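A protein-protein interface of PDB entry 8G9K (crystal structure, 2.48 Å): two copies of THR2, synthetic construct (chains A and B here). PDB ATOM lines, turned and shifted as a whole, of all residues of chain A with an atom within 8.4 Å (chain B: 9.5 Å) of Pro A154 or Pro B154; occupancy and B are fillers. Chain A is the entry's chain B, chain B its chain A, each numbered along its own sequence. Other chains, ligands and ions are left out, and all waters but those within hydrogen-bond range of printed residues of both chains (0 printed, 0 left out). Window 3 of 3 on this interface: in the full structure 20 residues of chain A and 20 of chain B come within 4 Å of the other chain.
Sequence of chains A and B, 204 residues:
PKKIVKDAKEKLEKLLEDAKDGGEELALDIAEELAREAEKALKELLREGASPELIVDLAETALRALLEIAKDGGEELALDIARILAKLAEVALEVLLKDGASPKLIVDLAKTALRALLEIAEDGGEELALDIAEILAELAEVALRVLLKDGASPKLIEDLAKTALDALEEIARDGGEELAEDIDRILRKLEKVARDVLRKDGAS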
ATOM      1  N   LEU A 144     -28.807 -39.324 -15.041  1.00  0.00           N
ATOM      2  CA  LEU A 144     -29.119 -38.037 -14.424  1.00  0.00           C
ATOM      3  C   LEU A 144     -29.897 -38.216 -13.128  1.00  0.00           C
ATOM      4  O   LEU A 144     -29.658 -37.500 -12.147  1.00  0.00           O
ATOM      5  CB  LEU A 144     -29.903 -37.161 -15.401  1.00  0.00           C
ATOM      6  CG  LEU A 144     -29.143 -36.629 -16.619  1.00  0.00           C
ATOM      7  CD1 LEU A 144     -30.087 -35.895 -17.558  1.00  0.00           C
ATOM      8  CD2 LEU A 144     -27.999 -35.725 -16.190  1.00  0.00           C
ATOM      9  N   LEU A 147     -27.540 -39.504 -10.467  1.00  0.00           N
ATOM     10  CA  LEU A 147     -26.760 -38.387  -9.940  1.00  0.00           C
ATOM     11  C   LEU A 147     -27.570 -37.575  -8.939  1.00  0.00           C
ATOM     12  O   LEU A 147     -27.041 -37.139  -7.909  1.00  0.00           O
ATOM     13  CB  LEU A 147     -26.281 -37.490 -11.081  1.00  0.00           C
ATOM     14  CG  LEU A 147     -24.987 -37.888 -11.789  1.00  0.00           C
ATOM     15  CD1 LEU A 147     -24.605 -36.831 -12.808  1.00  0.00           C
ATOM     16  CD2 LEU A 147     -23.872 -38.085 -10.778  1.00  0.00           C
ATOM     17  N   LEU A 148     -28.854 -37.356  -9.229  1.00  0.00           N
ATOM     18  CA  LEU A 148     -29.706 -36.609  -8.310  1.00  0.00           C
ATOM     19  C   LEU A 148     -29.858 -37.340  -6.982  1.00  0.00           C
ATOM     20  O   LEU A 148     -29.794 -36.720  -5.914  1.00  0.00           O
ATOM     21  CB  LEU A 148     -31.074 -36.362  -8.946  1.00  0.00           C
ATOM     22  CG  LEU A 148     -32.043 -35.485  -8.152  1.00  0.00           C
ATOM     23  CD1 LEU A 148     -31.528 -34.057  -8.070  1.00  0.00           C
ATOM     24  CD2 LEU A 148     -33.429 -35.526  -8.776  1.00  0.00           C
ATOM     25  N   GLY A 151     -26.764 -37.128  -4.568  1.00  0.00           N
ATOM     26  CA  GLY A 151     -26.414 -35.854  -3.982  1.00  0.00           C
ATOM     27  C   GLY A 151     -25.510 -34.989  -4.827  1.00  0.00           C
ATOM     28  O   GLY A 151     -24.910 -34.046  -4.297  1.00  0.00           O
ATOM     29  N   ALA A 152     -25.397 -35.272  -6.123  1.00  0.00           N
ATOM     30  CA  ALA A 152     -24.505 -34.523  -6.994  1.00  0.00           C
ATOM     31  C   ALA A 152     -24.937 -33.063  -7.088  1.00  0.00           C
ATOM     32  O   ALA A 152     -26.080 -32.700  -6.802  1.00  0.00           O
ATOM     33  CB  ALA A 152     -24.469 -35.151  -8.387  1.00  0.00           C
ATOM     34  N   SER A 153     -23.994 -32.218  -7.493  1.00  0.00           N
ATOM     35  CA  SER A 153     -24.255 -30.798  -7.642  1.00  0.00           C
ATOM     36  C   SER A 153     -24.867 -30.510  -9.009  1.00  0.00           C
ATOM     37  O   SER A 153     -24.751 -31.318  -9.934  1.00  0.00           O
ATOM     38  CB  SER A 153     -22.961 -30.010  -7.466  1.00  0.00           C
ATOM     39  OG  SER A 153     -22.007 -30.368  -8.451  1.00  0.00           O
ATOM     40  N   PRO A 154     -25.544 -29.367  -9.159  1.00  0.00           N
ATOM     41  CA  PRO A 154     -26.048 -28.995 -10.492  1.00  0.00           C
ATOM     42  C   PRO A 154     -24.954 -28.875 -11.538  1.00  0.00           C
ATOM     43  O   PRO A 154     -25.223 -29.088 -12.728  1.00  0.00           O
ATOM     44  CB  PRO A 154     -26.738 -27.647 -10.238  1.00  0.00           C
ATOM     45  CG  PRO A 154     -27.135 -27.700  -8.801  1.00  0.00           C
ATOM     46  CD  PRO A 154     -26.034 -28.456  -8.110  1.00  0.00           C
ATOM     47  N   LYS A 155     -23.728 -28.544 -11.130  1.00  0.00           N
ATOM     48  CA  LYS A 155     -22.623 -28.450 -12.079  1.00  0.00           C
ATOM     49  C   LYS A 155     -22.371 -29.788 -12.763  1.00  0.00           C
ATOM     50  O   LYS A 155     -22.277 -29.863 -13.994  1.00  0.00           O
ATOM     51  CB  LYS A 155     -21.364 -27.961 -11.361  1.00  0.00           C
ATOM     52  CG  LYS A 155     -20.141 -27.837 -12.247  1.00  0.00           C
ATOM     53  CD  LYS A 155     -18.966 -27.251 -11.479  1.00  0.00           C
ATOM     54  CE  LYS A 155     -17.779 -26.991 -12.393  1.00  0.00           C
ATOM     55  NZ  LYS A 155     -16.662 -26.311 -11.679  1.00  0.00           N
ATOM     56  N   LEU A 156     -22.265 -30.862 -11.977  1.00  0.00           N
ATOM     57  CA  LEU A 156     -21.997 -32.175 -12.551  1.00  0.00           C
ATOM     58  C   LEU A 156     -23.210 -32.732 -13.283  1.00  0.00           C
ATOM     59  O   LEU A 156     -23.055 -33.443 -14.283  1.00  0.00           O
ATOM     60  CB  LEU A 156     -21.546 -33.140 -11.456  1.00  0.00           C
ATOM     61  CG  LEU A 156     -20.150 -32.845 -10.909  1.00  0.00           C
ATOM     62  CD1 LEU A 156     -19.841 -33.722  -9.709  1.00  0.00           C
ATOM     63  CD2 LEU A 156     -19.114 -33.041 -12.004  1.00  0.00           C
ATOM     64  N   ILE A 157     -24.418 -32.428 -12.806  1.00  0.00           N
ATOM     65  CA  ILE A 157     -25.624 -32.878 -13.495  1.00  0.00           C
ATOM     66  C   ILE A 157     -25.736 -32.206 -14.858  1.00  0.00           C
ATOM     67  O   ILE A 157     -25.996 -32.862 -15.873  1.00  0.00           O
ATOM     68  CB  ILE A 157     -26.870 -32.614 -12.629  1.00  0.00           C
ATOM     69  CG1 ILE A 157     -26.814 -33.451 -11.350  1.00  0.00           C
ATOM     70  CG2 ILE A 157     -28.138 -32.921 -13.411  1.00  0.00           C
ATOM     71  CD1 ILE A 157     -27.954 -33.181 -10.394  1.00  0.00           C
ATOM     72  N   GLU A 158     -25.535 -30.886 -14.902  1.00  0.00           N
ATOM     73  CA  GLU A 158     -25.543 -30.182 -16.181  1.00  0.00           C
ATOM     74  C   GLU A 158     -24.396 -30.640 -17.073  1.00  0.00           C
ATOM     75  O   GLU A 158     -24.533 -30.654 -18.302  1.00  0.00           O
ATOM     76  CB  GLU A 158     -25.474 -28.672 -15.952  1.00  0.00           C
ATOM     77  CG  GLU A 158     -25.534 -27.844 -17.228  1.00  0.00           C
ATOM     78  CD  GLU A 158     -25.397 -26.357 -16.969  1.00  0.00           C
ATOM     79  OE1 GLU A 158     -25.606 -25.933 -15.812  1.00  0.00           O
ATOM     80  OE2 GLU A 158     -25.074 -25.613 -17.919  1.00  0.00           O
ATOM     81  N   ASP A 159     -23.267 -31.025 -16.474  1.00  0.00           N
ATOM     82  CA  ASP A 159     -22.141 -31.532 -17.253  1.00  0.00           C
ATOM     83  C   ASP A 159     -22.508 -32.825 -17.972  1.00  0.00           C
ATOM     84  O   ASP A 159     -22.285 -32.964 -19.181  1.00  0.00           O
ATOM     85  CB  ASP A 159     -20.931 -31.747 -16.342  1.00  0.00           C
ATOM     86  CG  ASP A 159     -19.779 -32.426 -17.056  1.00  0.00           C
ATOM     87  OD1 ASP A 159     -19.254 -31.839 -18.024  1.00  0.00           O
ATOM     88  OD2 ASP A 159     -19.399 -33.545 -16.650  1.00  0.00           O
ATOM     89  N   LEU A 160     -23.073 -33.788 -17.239  1.00  0.00           N
ATOM     90  CA  LEU A 160     -23.471 -35.049 -17.857  1.00  0.00           C
ATOM     91  C   LEU A 160     -24.585 -34.838 -18.876  1.00  0.00           C
ATOM     92  O   LEU A 160     -24.636 -35.526 -19.903  1.00  0.00           O
ATOM     93  CB  LEU A 160     -23.912 -36.043 -16.785  1.00  0.00           C
ATOM     94  CG  LEU A 160     -24.356 -37.419 -17.281  1.00  0.00           C
ATOM     95  CD1 LEU A 160     -23.225 -38.102 -18.033  1.00  0.00           C
ATOM     96  CD2 LEU A 160     -24.826 -38.272 -16.121  1.00  0.00           C
ATOM     97  N   ALA A 161     -25.483 -33.888 -18.610  1.00  0.00           N
ATOM     98  CA  ALA A 161     -26.565 -33.603 -19.548  1.00  0.00           C
ATOM     99  C   ALA A 161     -26.022 -33.076 -20.870  1.00  0.00           C
ATOM    100  O   ALA A 161     -26.455 -33.502 -21.947  1.00  0.00           O
ATOM    101  CB  ALA A 161     -27.544 -32.603 -18.933  1.00  0.00           C
ATOM    102  N   ALA A 194     -33.579 -33.068 -18.067  1.00  0.00           N
ATOM    103  CA  ALA A 194     -32.461 -32.407 -17.403  1.00  0.00           C
ATOM    104  C   ALA A 194     -32.920 -31.156 -16.663  1.00  0.00           C
ATOM    105  O   ALA A 194     -32.410 -30.846 -15.580  1.00  0.00           O
ATOM    106  CB  ALA A 194     -31.375 -32.060 -18.421  1.00  0.00           C
ATOM    107  N   VAL A 197     -34.666 -32.349 -13.397  1.00  0.00           N
ATOM    108  CA  VAL A 197     -33.716 -32.840 -12.403  1.00  0.00           C
ATOM    109  C   VAL A 197     -32.960 -31.680 -11.767  1.00  0.00           C
ATOM    110  O   VAL A 197     -32.687 -31.686 -10.560  1.00  0.00           O
ATOM    111  CB  VAL A 197     -32.760 -33.863 -13.045  1.00  0.00           C
ATOM    112  CG1 VAL A 197     -31.664 -34.263 -12.069  1.00  0.00           C
ATOM    113  CG2 VAL A 197     -33.531 -35.087 -13.510  1.00  0.00           C
ATOM    114  N   LEU A 198     -32.622 -30.661 -12.560  1.00  0.00           N
ATOM    115  CA  LEU A 198     -31.881 -29.524 -12.027  1.00  0.00           C
ATOM    116  C   LEU A 198     -32.752 -28.636 -11.147  1.00  0.00           C
ATOM    117  O   LEU A 198     -32.243 -28.014 -10.207  1.00  0.00           O
ATOM    118  CB  LEU A 198     -31.278 -28.710 -13.171  1.00  0.00           C
ATOM    119  CG  LEU A 198     -30.054 -29.328 -13.850  1.00  0.00           C
ATOM    120  CD1 LEU A 198     -29.704 -28.578 -15.124  1.00  0.00           C
ATOM    121  CD2 LEU A 198     -28.875 -29.336 -12.894  1.00  0.00           C
ATOM    122  N   ARG A 199     -34.055 -28.558 -11.430  1.00  0.00           N
ATOM    123  CA  ARG A 199     -34.933 -27.720 -10.616  1.00  0.00           C
ATOM    124  C   ARG A 199     -35.124 -28.306  -9.223  1.00  0.00           C
ATOM    125  O   ARG A 199     -35.208 -27.563  -8.237  1.00  0.00           O
ATOM    126  CB  ARG A 199     -36.278 -27.528 -11.314  1.00  0.00           C
ATOM    127  CG  ARG A 199     -36.225 -26.540 -12.467  1.00  0.00           C
ATOM    128  CD  ARG A 199     -37.603 -26.251 -13.031  1.00  0.00           C
ATOM    129  NE  ARG A 199     -37.547 -25.234 -14.077  1.00  0.00           N
ATOM    130  CZ  ARG A 199     -38.612 -24.724 -14.688  1.00  0.00           C
ATOM    131  NH1 ARG A 199     -39.828 -25.135 -14.358  1.00  0.00           N
ATOM    132  NH2 ARG A 199     -38.459 -23.800 -15.627  1.00  0.00           N
ATOM    133  N   LYS A 200     -35.196 -29.634  -9.118  1.00  0.00           N
ATOM    134  CA  LYS A 200     -35.210 -30.283  -7.812  1.00  0.00           C
ATOM    135  C   LYS A 200     -33.879 -30.147  -7.085  1.00  0.00           C
ATOM    136  O   LYS A 200     -33.808 -30.452  -5.889  1.00  0.00           O
ATOM    137  CB  LYS A 200     -35.568 -31.763  -7.965  1.00  0.00           C
ATOM    138  CG  LYS A 200     -36.870 -32.013  -8.707  1.00  0.00           C
ATOM    139  CD  LYS A 200     -37.034 -33.483  -9.068  1.00  0.00           C
ATOM    140  CE  LYS A 200     -37.149 -34.356  -7.829  1.00  0.00           C
ATOM    141  NZ  LYS A 200     -37.367 -35.788  -8.183  1.00  0.00           N
ATOM    142  N   ASP A 201     -32.836 -29.696  -7.774  1.00  0.00           N
ATOM    143  CA  ASP A 201     -31.513 -29.533  -7.190  1.00  0.00           C
ATOM    144  C   ASP A 201     -31.073 -28.074  -7.285  1.00  0.00           C
ATOM    145  O   ASP A 201     -31.460 -27.242  -6.465  1.00  0.00           O
ATOM    146  CB  ASP A 201     -30.508 -30.443  -7.896  1.00  0.00           C
ATOM    147  CG  ASP A 201     -29.224 -30.627  -7.108  1.00  0.00           C
ATOM    148  OD1 ASP A 201     -28.866 -29.735  -6.311  1.00  0.00           O
ATOM    149  OD2 ASP A 201     -28.568 -31.672  -7.292  1.00  0.00           O
ATOM    150  N   PRO B 103     -21.554 -37.698  -1.256  1.00  0.00           N
ATOM    151  CA  PRO B 103     -21.702 -36.589  -0.301  1.00  0.00           C
ATOM    152  C   PRO B 103     -22.544 -36.950   0.909  1.00  0.00           C
ATOM    153  O   PRO B 103     -22.306 -36.412   1.999  1.00  0.00           O
ATOM    154  CB  PRO B 103     -22.362 -35.489  -1.142  1.00  0.00           C
ATOM    155  CG  PRO B 103     -22.025 -35.832  -2.556  1.00  0.00           C
ATOM    156  CD  PRO B 103     -22.007 -37.327  -2.608  1.00  0.00           C
ATOM    157  N   VAL B 107     -21.568 -36.381   4.788  1.00  0.00           N
ATOM    158  CA  VAL B 107     -22.438 -35.641   5.700  1.00  0.00           C
ATOM    159  C   VAL B 107     -22.748 -36.471   6.937  1.00  0.00           C
ATOM    160  O   VAL B 107     -22.761 -35.954   8.063  1.00  0.00           O
ATOM    161  CB  VAL B 107     -23.729 -35.211   4.978  1.00  0.00           C
ATOM    162  CG1 VAL B 107     -24.751 -34.692   5.979  1.00  0.00           C
ATOM    163  CG2 VAL B 107     -23.429 -34.154   3.939  1.00  0.00           C
ATOM    164  N   LEU B 144     -17.274 -29.091   5.471  1.00  0.00           N
ATOM    165  CA  LEU B 144     -17.950 -28.328   4.425  1.00  0.00           C
ATOM    166  C   LEU B 144     -17.085 -28.207   3.177  1.00  0.00           C
ATOM    167  O   LEU B 144     -17.587 -28.315   2.052  1.00  0.00           O
ATOM    168  CB  LEU B 144     -18.328 -26.942   4.945  1.00  0.00           C
ATOM    169  CG  LEU B 144     -19.523 -26.866   5.895  1.00  0.00           C
ATOM    170  CD1 LEU B 144     -19.677 -25.455   6.439  1.00  0.00           C
ATOM    171  CD2 LEU B 144     -20.793 -27.311   5.188  1.00  0.00           C
ATOM    172  N   LEU B 147     -16.963 -31.553   1.425  1.00  0.00           N
ATOM    173  CA  LEU B 147     -18.209 -31.727   0.680  1.00  0.00           C
ATOM    174  C   LEU B 147     -18.157 -31.007  -0.660  1.00  0.00           C
ATOM    175  O   LEU B 147     -18.574 -31.558  -1.686  1.00  0.00           O
ATOM    176  CB  LEU B 147     -19.393 -31.214   1.498  1.00  0.00           C
ATOM    177  CG  LEU B 147     -20.105 -32.164   2.456  1.00  0.00           C
ATOM    178  CD1 LEU B 147     -21.308 -31.453   3.041  1.00  0.00           C
ATOM    179  CD2 LEU B 147     -20.526 -33.441   1.744  1.00  0.00           C
ATOM    180  N   LEU B 148     -17.650 -29.772  -0.668  1.00  0.00           N
ATOM    181  CA  LEU B 148     -17.551 -29.016  -1.913  1.00  0.00           C
ATOM    182  C   LEU B 148     -16.642 -29.718  -2.914  1.00  0.00           C
ATOM    183  O   LEU B 148     -16.955 -29.782  -4.109  1.00  0.00           O
ATOM    184  CB  LEU B 148     -17.043 -27.603  -1.624  1.00  0.00           C
ATOM    185  CG  LEU B 148     -17.052 -26.607  -2.786  1.00  0.00           C
ATOM    186  CD1 LEU B 148     -18.478 -26.289  -3.208  1.00  0.00           C
ATOM    187  CD2 LEU B 148     -16.305 -25.339  -2.402  1.00  0.00           C
ATOM    188  N   GLY B 151     -18.248 -32.702  -4.893  1.00  0.00           N
ATOM    189  CA  GLY B 151     -19.382 -32.473  -5.767  1.00  0.00           C
ATOM    190  C   GLY B 151     -20.725 -32.502  -5.076  1.00  0.00           C
ATOM    191  O   GLY B 151     -21.720 -32.906  -5.686  1.00  0.00           O
ATOM    192  N   ALA B 152     -20.781 -32.089  -3.813  1.00  0.00           N
ATOM    193  CA  ALA B 152     -22.036 -32.072  -3.079  1.00  0.00           C
ATOM    194  C   ALA B 152     -22.944 -30.960  -3.590  1.00  0.00           C
ATOM    195  O   ALA B 152     -22.487 -29.938  -4.109  1.00  0.00           O
ATOM    196  CB  ALA B 152     -21.778 -31.890  -1.583  1.00  0.00           C
ATOM    197  N   SER B 153     -24.246 -31.174  -3.441  1.00  0.00           N
ATOM    198  CA  SER B 153     -25.237 -30.190  -3.836  1.00  0.00           C
ATOM    199  C   SER B 153     -25.333 -29.089  -2.785  1.00  0.00           C
ATOM    200  O   SER B 153     -24.851 -29.248  -1.661  1.00  0.00           O
ATOM    201  CB  SER B 153     -26.592 -30.864  -4.021  1.00  0.00           C
ATOM    202  OG  SER B 153     -27.077 -31.370  -2.789  1.00  0.00           O
ATOM    203  N   PRO B 154     -25.936 -27.948  -3.131  1.00  0.00           N
ATOM    204  CA  PRO B 154     -26.186 -26.925  -2.101  1.00  0.00           C
ATOM    205  C   PRO B 154     -27.050 -27.423  -0.956  1.00  0.00           C
ATOM    206  O   PRO B 154     -26.871 -26.973   0.182  1.00  0.00           O
ATOM    207  CB  PRO B 154     -26.878 -25.803  -2.886  1.00  0.00           C
ATOM    208  CG  PRO B 154     -26.383 -25.969  -4.279  1.00  0.00           C
ATOM    209  CD  PRO B 154     -26.245 -27.451  -4.483  1.00  0.00           C
ATOM    210  N   LYS B 155     -27.978 -28.347  -1.222  1.00  0.00           N
ATOM    211  CA  LYS B 155     -28.864 -28.843  -0.172  1.00  0.00           C
ATOM    212  C   LYS B 155     -28.080 -29.580   0.907  1.00  0.00           C
ATOM    213  O   LYS B 155     -28.252 -29.318   2.104  1.00  0.00           O
ATOM    214  CB  LYS B 155     -29.934 -29.754  -0.778  1.00  0.00           C
ATOM    215  N   LEU B 156     -27.209 -30.507   0.501  1.00  0.00           N
ATOM    216  CA  LEU B 156     -26.420 -31.257   1.474  1.00  0.00           C
ATOM    217  C   LEU B 156     -25.429 -30.355   2.198  1.00  0.00           C
ATOM    218  O   LEU B 156     -25.214 -30.507   3.407  1.00  0.00           O
ATOM    219  CB  LEU B 156     -25.690 -32.405   0.779  1.00  0.00           C
ATOM    220  CG  LEU B 156     -26.584 -33.507   0.209  1.00  0.00           C
ATOM    221  CD1 LEU B 156     -25.772 -34.472  -0.635  1.00  0.00           C
ATOM    222  CD2 LEU B 156     -27.292 -34.244   1.333  1.00  0.00           C
ATOM    223  N   ILE B 157     -24.815 -29.413   1.478  1.00  0.00           N
ATOM    224  CA  ILE B 157     -23.867 -28.493   2.103  1.00  0.00           C
ATOM    225  C   ILE B 157     -24.577 -27.611   3.122  1.00  0.00           C
ATOM    226  O   ILE B 157     -24.108 -27.433   4.252  1.00  0.00           O
ATOM    227  CB  ILE B 157     -23.148 -27.650   1.034  1.00  0.00           C
ATOM    228  CG1 ILE B 157     -22.281 -28.539   0.141  1.00  0.00           C
ATOM    229  CG2 ILE B 157     -22.304 -26.564   1.687  1.00  0.00           C
ATOM    230  CD1 ILE B 157     -21.591 -27.789  -0.974  1.00  0.00           C
ATOM    231  N   GLU B 158     -25.723 -27.044   2.736  1.00  0.00           N
ATOM    232  CA  GLU B 158     -26.487 -26.218   3.667  1.00  0.00           C
ATOM    233  C   GLU B 158     -27.032 -27.044   4.825  1.00  0.00           C
ATOM    234  O   GLU B 158     -27.220 -26.519   5.928  1.00  0.00           O
ATOM    235  CB  GLU B 158     -27.627 -25.512   2.928  1.00  0.00           C
ATOM    236  CG  GLU B 158     -28.110 -24.229   3.591  1.00  0.00           C
ATOM    237  CD  GLU B 158     -29.130 -23.484   2.748  1.00  0.00           C
ATOM    238  OE1 GLU B 158     -30.025 -24.140   2.174  1.00  0.00           O
ATOM    239  OE2 GLU B 158     -29.031 -22.242   2.653  1.00  0.00           O
ATOM    240  N   ASP B 159     -27.286 -28.335   4.595  1.00  0.00           N
ATOM    241  CA  ASP B 159     -27.761 -29.208   5.665  1.00  0.00           C
ATOM    242  C   ASP B 159     -26.686 -29.411   6.726  1.00  0.00           C
ATOM    243  O   ASP B 159     -26.955 -29.296   7.928  1.00  0.00           O
ATOM    244  CB  ASP B 159     -28.207 -30.551   5.088  1.00  0.00           C
ATOM    245  CG  ASP B 159     -28.641 -31.528   6.159  1.00  0.00           C
ATOM    246  OD1 ASP B 159     -29.511 -31.158   6.976  1.00  0.00           O
ATOM    247  OD2 ASP B 159     -28.118 -32.662   6.185  1.00  0.00           O
ATOM    248  N   LEU B 160     -25.462 -29.725   6.298  1.00  0.00           N
ATOM    249  CA  LEU B 160     -24.360 -29.884   7.243  1.00  0.00           C
ATOM    250  C   LEU B 160     -24.056 -28.575   7.962  1.00  0.00           C
ATOM    251  O   LEU B 160     -23.698 -28.576   9.147  1.00  0.00           O
ATOM    252  CB  LEU B 160     -23.119 -30.395   6.517  1.00  0.00           C
ATOM    253  CG  LEU B 160     -21.842 -30.460   7.354  1.00  0.00           C
ATOM    254  CD1 LEU B 160     -22.026 -31.410   8.524  1.00  0.00           C
ATOM    255  CD2 LEU B 160     -20.661 -30.873   6.496  1.00  0.00           C
ATOM    256  N   ALA B 161     -24.187 -27.446   7.261  1.00  0.00           N
ATOM    257  CA  ALA B 161     -23.966 -26.147   7.888  1.00  0.00           C
ATOM    258  C   ALA B 161     -24.986 -25.888   8.991  1.00  0.00           C
ATOM    259  O   ALA B 161     -24.633 -25.433  10.086  1.00  0.00           O
ATOM    260  CB  ALA B 161     -24.023 -25.040   6.836  1.00  0.00           C
ATOM    261  N   LYS B 162     -26.261 -26.172   8.716  1.00  0.00           N
ATOM    262  CA  LYS B 162     -27.308 -25.988   9.717  1.00  0.00           C
ATOM    263  C   LYS B 162     -27.027 -26.810  10.969  1.00  0.00           C
ATOM    264  O   LYS B 162     -27.174 -26.318  12.094  1.00  0.00           O
ATOM    265  CB  LYS B 162     -28.665 -26.368   9.127  1.00  0.00           C
ATOM    266  CG  LYS B 162     -29.822 -26.270  10.104  1.00  0.00           C
ATOM    267  CD  LYS B 162     -31.050 -26.978   9.557  1.00  0.00           C
ATOM    268  CE  LYS B 162     -32.284 -26.657  10.379  1.00  0.00           C
ATOM    269  NZ  LYS B 162     -32.102 -27.007  11.812  1.00  0.00           N
ATOM    270  N   ALA B 194     -19.709 -20.866   5.421  1.00  0.00           N
ATOM    271  CA  ALA B 194     -20.761 -21.582   4.706  1.00  0.00           C
ATOM    272  C   ALA B 194     -21.233 -20.799   3.487  1.00  0.00           C
ATOM    273  O   ALA B 194     -21.518 -21.388   2.437  1.00  0.00           O
ATOM    274  CB  ALA B 194     -21.933 -21.872   5.644  1.00  0.00           C
ATOM    275  N   VAL B 197     -18.589 -21.224   0.737  1.00  0.00           N
ATOM    276  CA  VAL B 197     -18.620 -22.556   0.140  1.00  0.00           C
ATOM    277  C   VAL B 197     -19.863 -22.728  -0.726  1.00  0.00           C
ATOM    278  O   VAL B 197     -19.807 -23.337  -1.802  1.00  0.00           O
ATOM    279  CB  VAL B 197     -18.537 -23.630   1.239  1.00  0.00           C
ATOM    280  CG1 VAL B 197     -18.789 -25.013   0.660  1.00  0.00           C
ATOM    281  CG2 VAL B 197     -17.179 -23.578   1.921  1.00  0.00           C
ATOM    282  N   LEU B 198     -21.001 -22.188  -0.281  1.00  0.00           N
ATOM    283  CA  LEU B 198     -22.235 -22.326  -1.050  1.00  0.00           C
ATOM    284  C   LEU B 198     -22.187 -21.533  -2.350  1.00  0.00           C
ATOM    285  O   LEU B 198     -22.844 -21.912  -3.328  1.00  0.00           O
ATOM    286  CB  LEU B 198     -23.432 -21.896  -0.204  1.00  0.00           C
ATOM    287  CG  LEU B 198     -23.920 -22.934   0.809  1.00  0.00           C
ATOM    288  CD1 LEU B 198     -24.877 -22.309   1.812  1.00  0.00           C
ATOM    289  CD2 LEU B 198     -24.581 -24.098   0.089  1.00  0.00           C
ATOM    290  N   ARG B 199     -21.429 -20.441  -2.388  1.00  0.00           N
ATOM    291  CA  ARG B 199     -21.259 -19.678  -3.620  1.00  0.00           C
ATOM    292  C   ARG B 199     -20.328 -20.409  -4.580  1.00  0.00           C
ATOM    293  O   ARG B 199     -19.432 -21.137  -4.154  1.00  0.00           O
ATOM    294  CB  ARG B 199     -20.713 -18.277  -3.326  1.00  0.00           C
ATOM    295  CG  ARG B 199     -21.776 -17.191  -3.217  1.00  0.00           C
ATOM    296  CD  ARG B 199     -22.730 -17.451  -2.063  1.00  0.00           C
ATOM    297  NE  ARG B 199     -23.556 -16.288  -1.756  1.00  0.00           N
ATOM    298  CZ  ARG B 199     -23.192 -15.309  -0.933  1.00  0.00           C
ATOM    299  NH1 ARG B 199     -22.011 -15.347  -0.334  1.00  0.00           N
ATOM    300  NH2 ARG B 199     -24.011 -14.289  -0.711  1.00  0.00           N
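Gly A151 touches Pro B103 (O to CG, 3.8 Å).
O of Gly A151 touches O of Gly B151 (3.7 Å).
O of Gly A151 touches CA of Ala B152 (3.7 Å).
CA of Gly A151 touches CD1 of Leu B156, at 3.7 Å.
Ala A152 touches Gly B151.
Ser B153 touches Ala A152 (CB to O, 3.4 Å).
O of Ala B152 touches CB of Ser A153, 3.4 Å away.
Pro A154 touches Pro B154 (CD to CD, 3.8 Å).
Ser B153 touches Asp A201.
Pro B154 touches Asp A201 (CD to OD1, 3.9 Å).
The backbone NH (N) of Ala A152 is in hydrogen-bond range of the backbone carbonyl oxygen (O) of Leu A147, 3.1 Å away.
The backbone carbonyl oxygen (O) of Leu B147 sits at hydrogen-bond distance from the backbone NH (N) of Ala B152, at 3.1 Å.
O of Ala A152 lies close to OD2 of Asp A201.
The backbone NH (N) of Leu B156 sits at hydrogen-bond distance from the side-chain hydroxyl (OG) of Ser B153 (3.4 Å).
The backbone NH (N) of Ser A153 sits at hydrogen-bond distance from the backbone carbonyl oxygen (O) of Gly B151, 3.0 Å away.
O of Gly A151 is in hydrogen-bond range of N of Ser B153, at 3.1 Å.
Gly A151 touches Ala B152, and with the chains exchanged Ala A152 touches Gly B151.
Gly A151 touches Ser B153, and with the chains exchanged Ser A153 touches Gly B151.
Ala A152 touches Ser B153, and with the chains exchanged Ser A153 touches Ala B152.
Pro A154 touches its own counterpart, Pro B154.
Of the 21 printed residues of chain B, 6 touch a printed residue of chain A.
Hydrophobic or aromatic side chains of chain B that line the printed part of chain A: Pro B103, Pro B154 and Leu B156.
Among the printed residues, no Asp or Glu carboxylate lies within 4 Å of a Lys or Arg side-chain nitrogen of the other chain.
Pro B154 touches just these residues of chain A: Pro A154 and Asp A201.
Printed residues of chain B within 4 Å of Ser A153: Gly B151, Ala B152 and Ser B153.
No residue of chain B comes within 4 Å of Ile A157.
Of the printed residues of chain A, Ser B153 touches Gly A151 (3.1 Å), Ala A152 (3.4 Å), Ser A153 (3.98 Å) and Asp A201 (3.4 Å).
No residue of chain A comes within 4 Å of Lys B155.
Of the printed residues of chain B, Gly A151 touches Pro B103 (3.8 Å), Gly B151 (3.7 Å), Ala B152 (3.7 Å), Ser B153 (3.1 Å) and Leu B156 (3.7 Å).
Of the printed residues of chain A, Pro B103 touches Gly A151.
Of the printed residues of chain A, Ala B152 touches Gly A151 (3.7 Å) and Ser A153 (3.4 Å).
Printed residues of chain A within 4 Å of Gly B151: Gly A151 (3.7 Å), Ala A152 (3.5 Å) and Ser A153 (3.0 Å).
The nearest residue of chain A that does not touch Pro B154 is Ser A153 (5.0 Å).
The nearest printed residue of chain A that does not touch Pro B103 is Ala A152 (4.9 Å).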
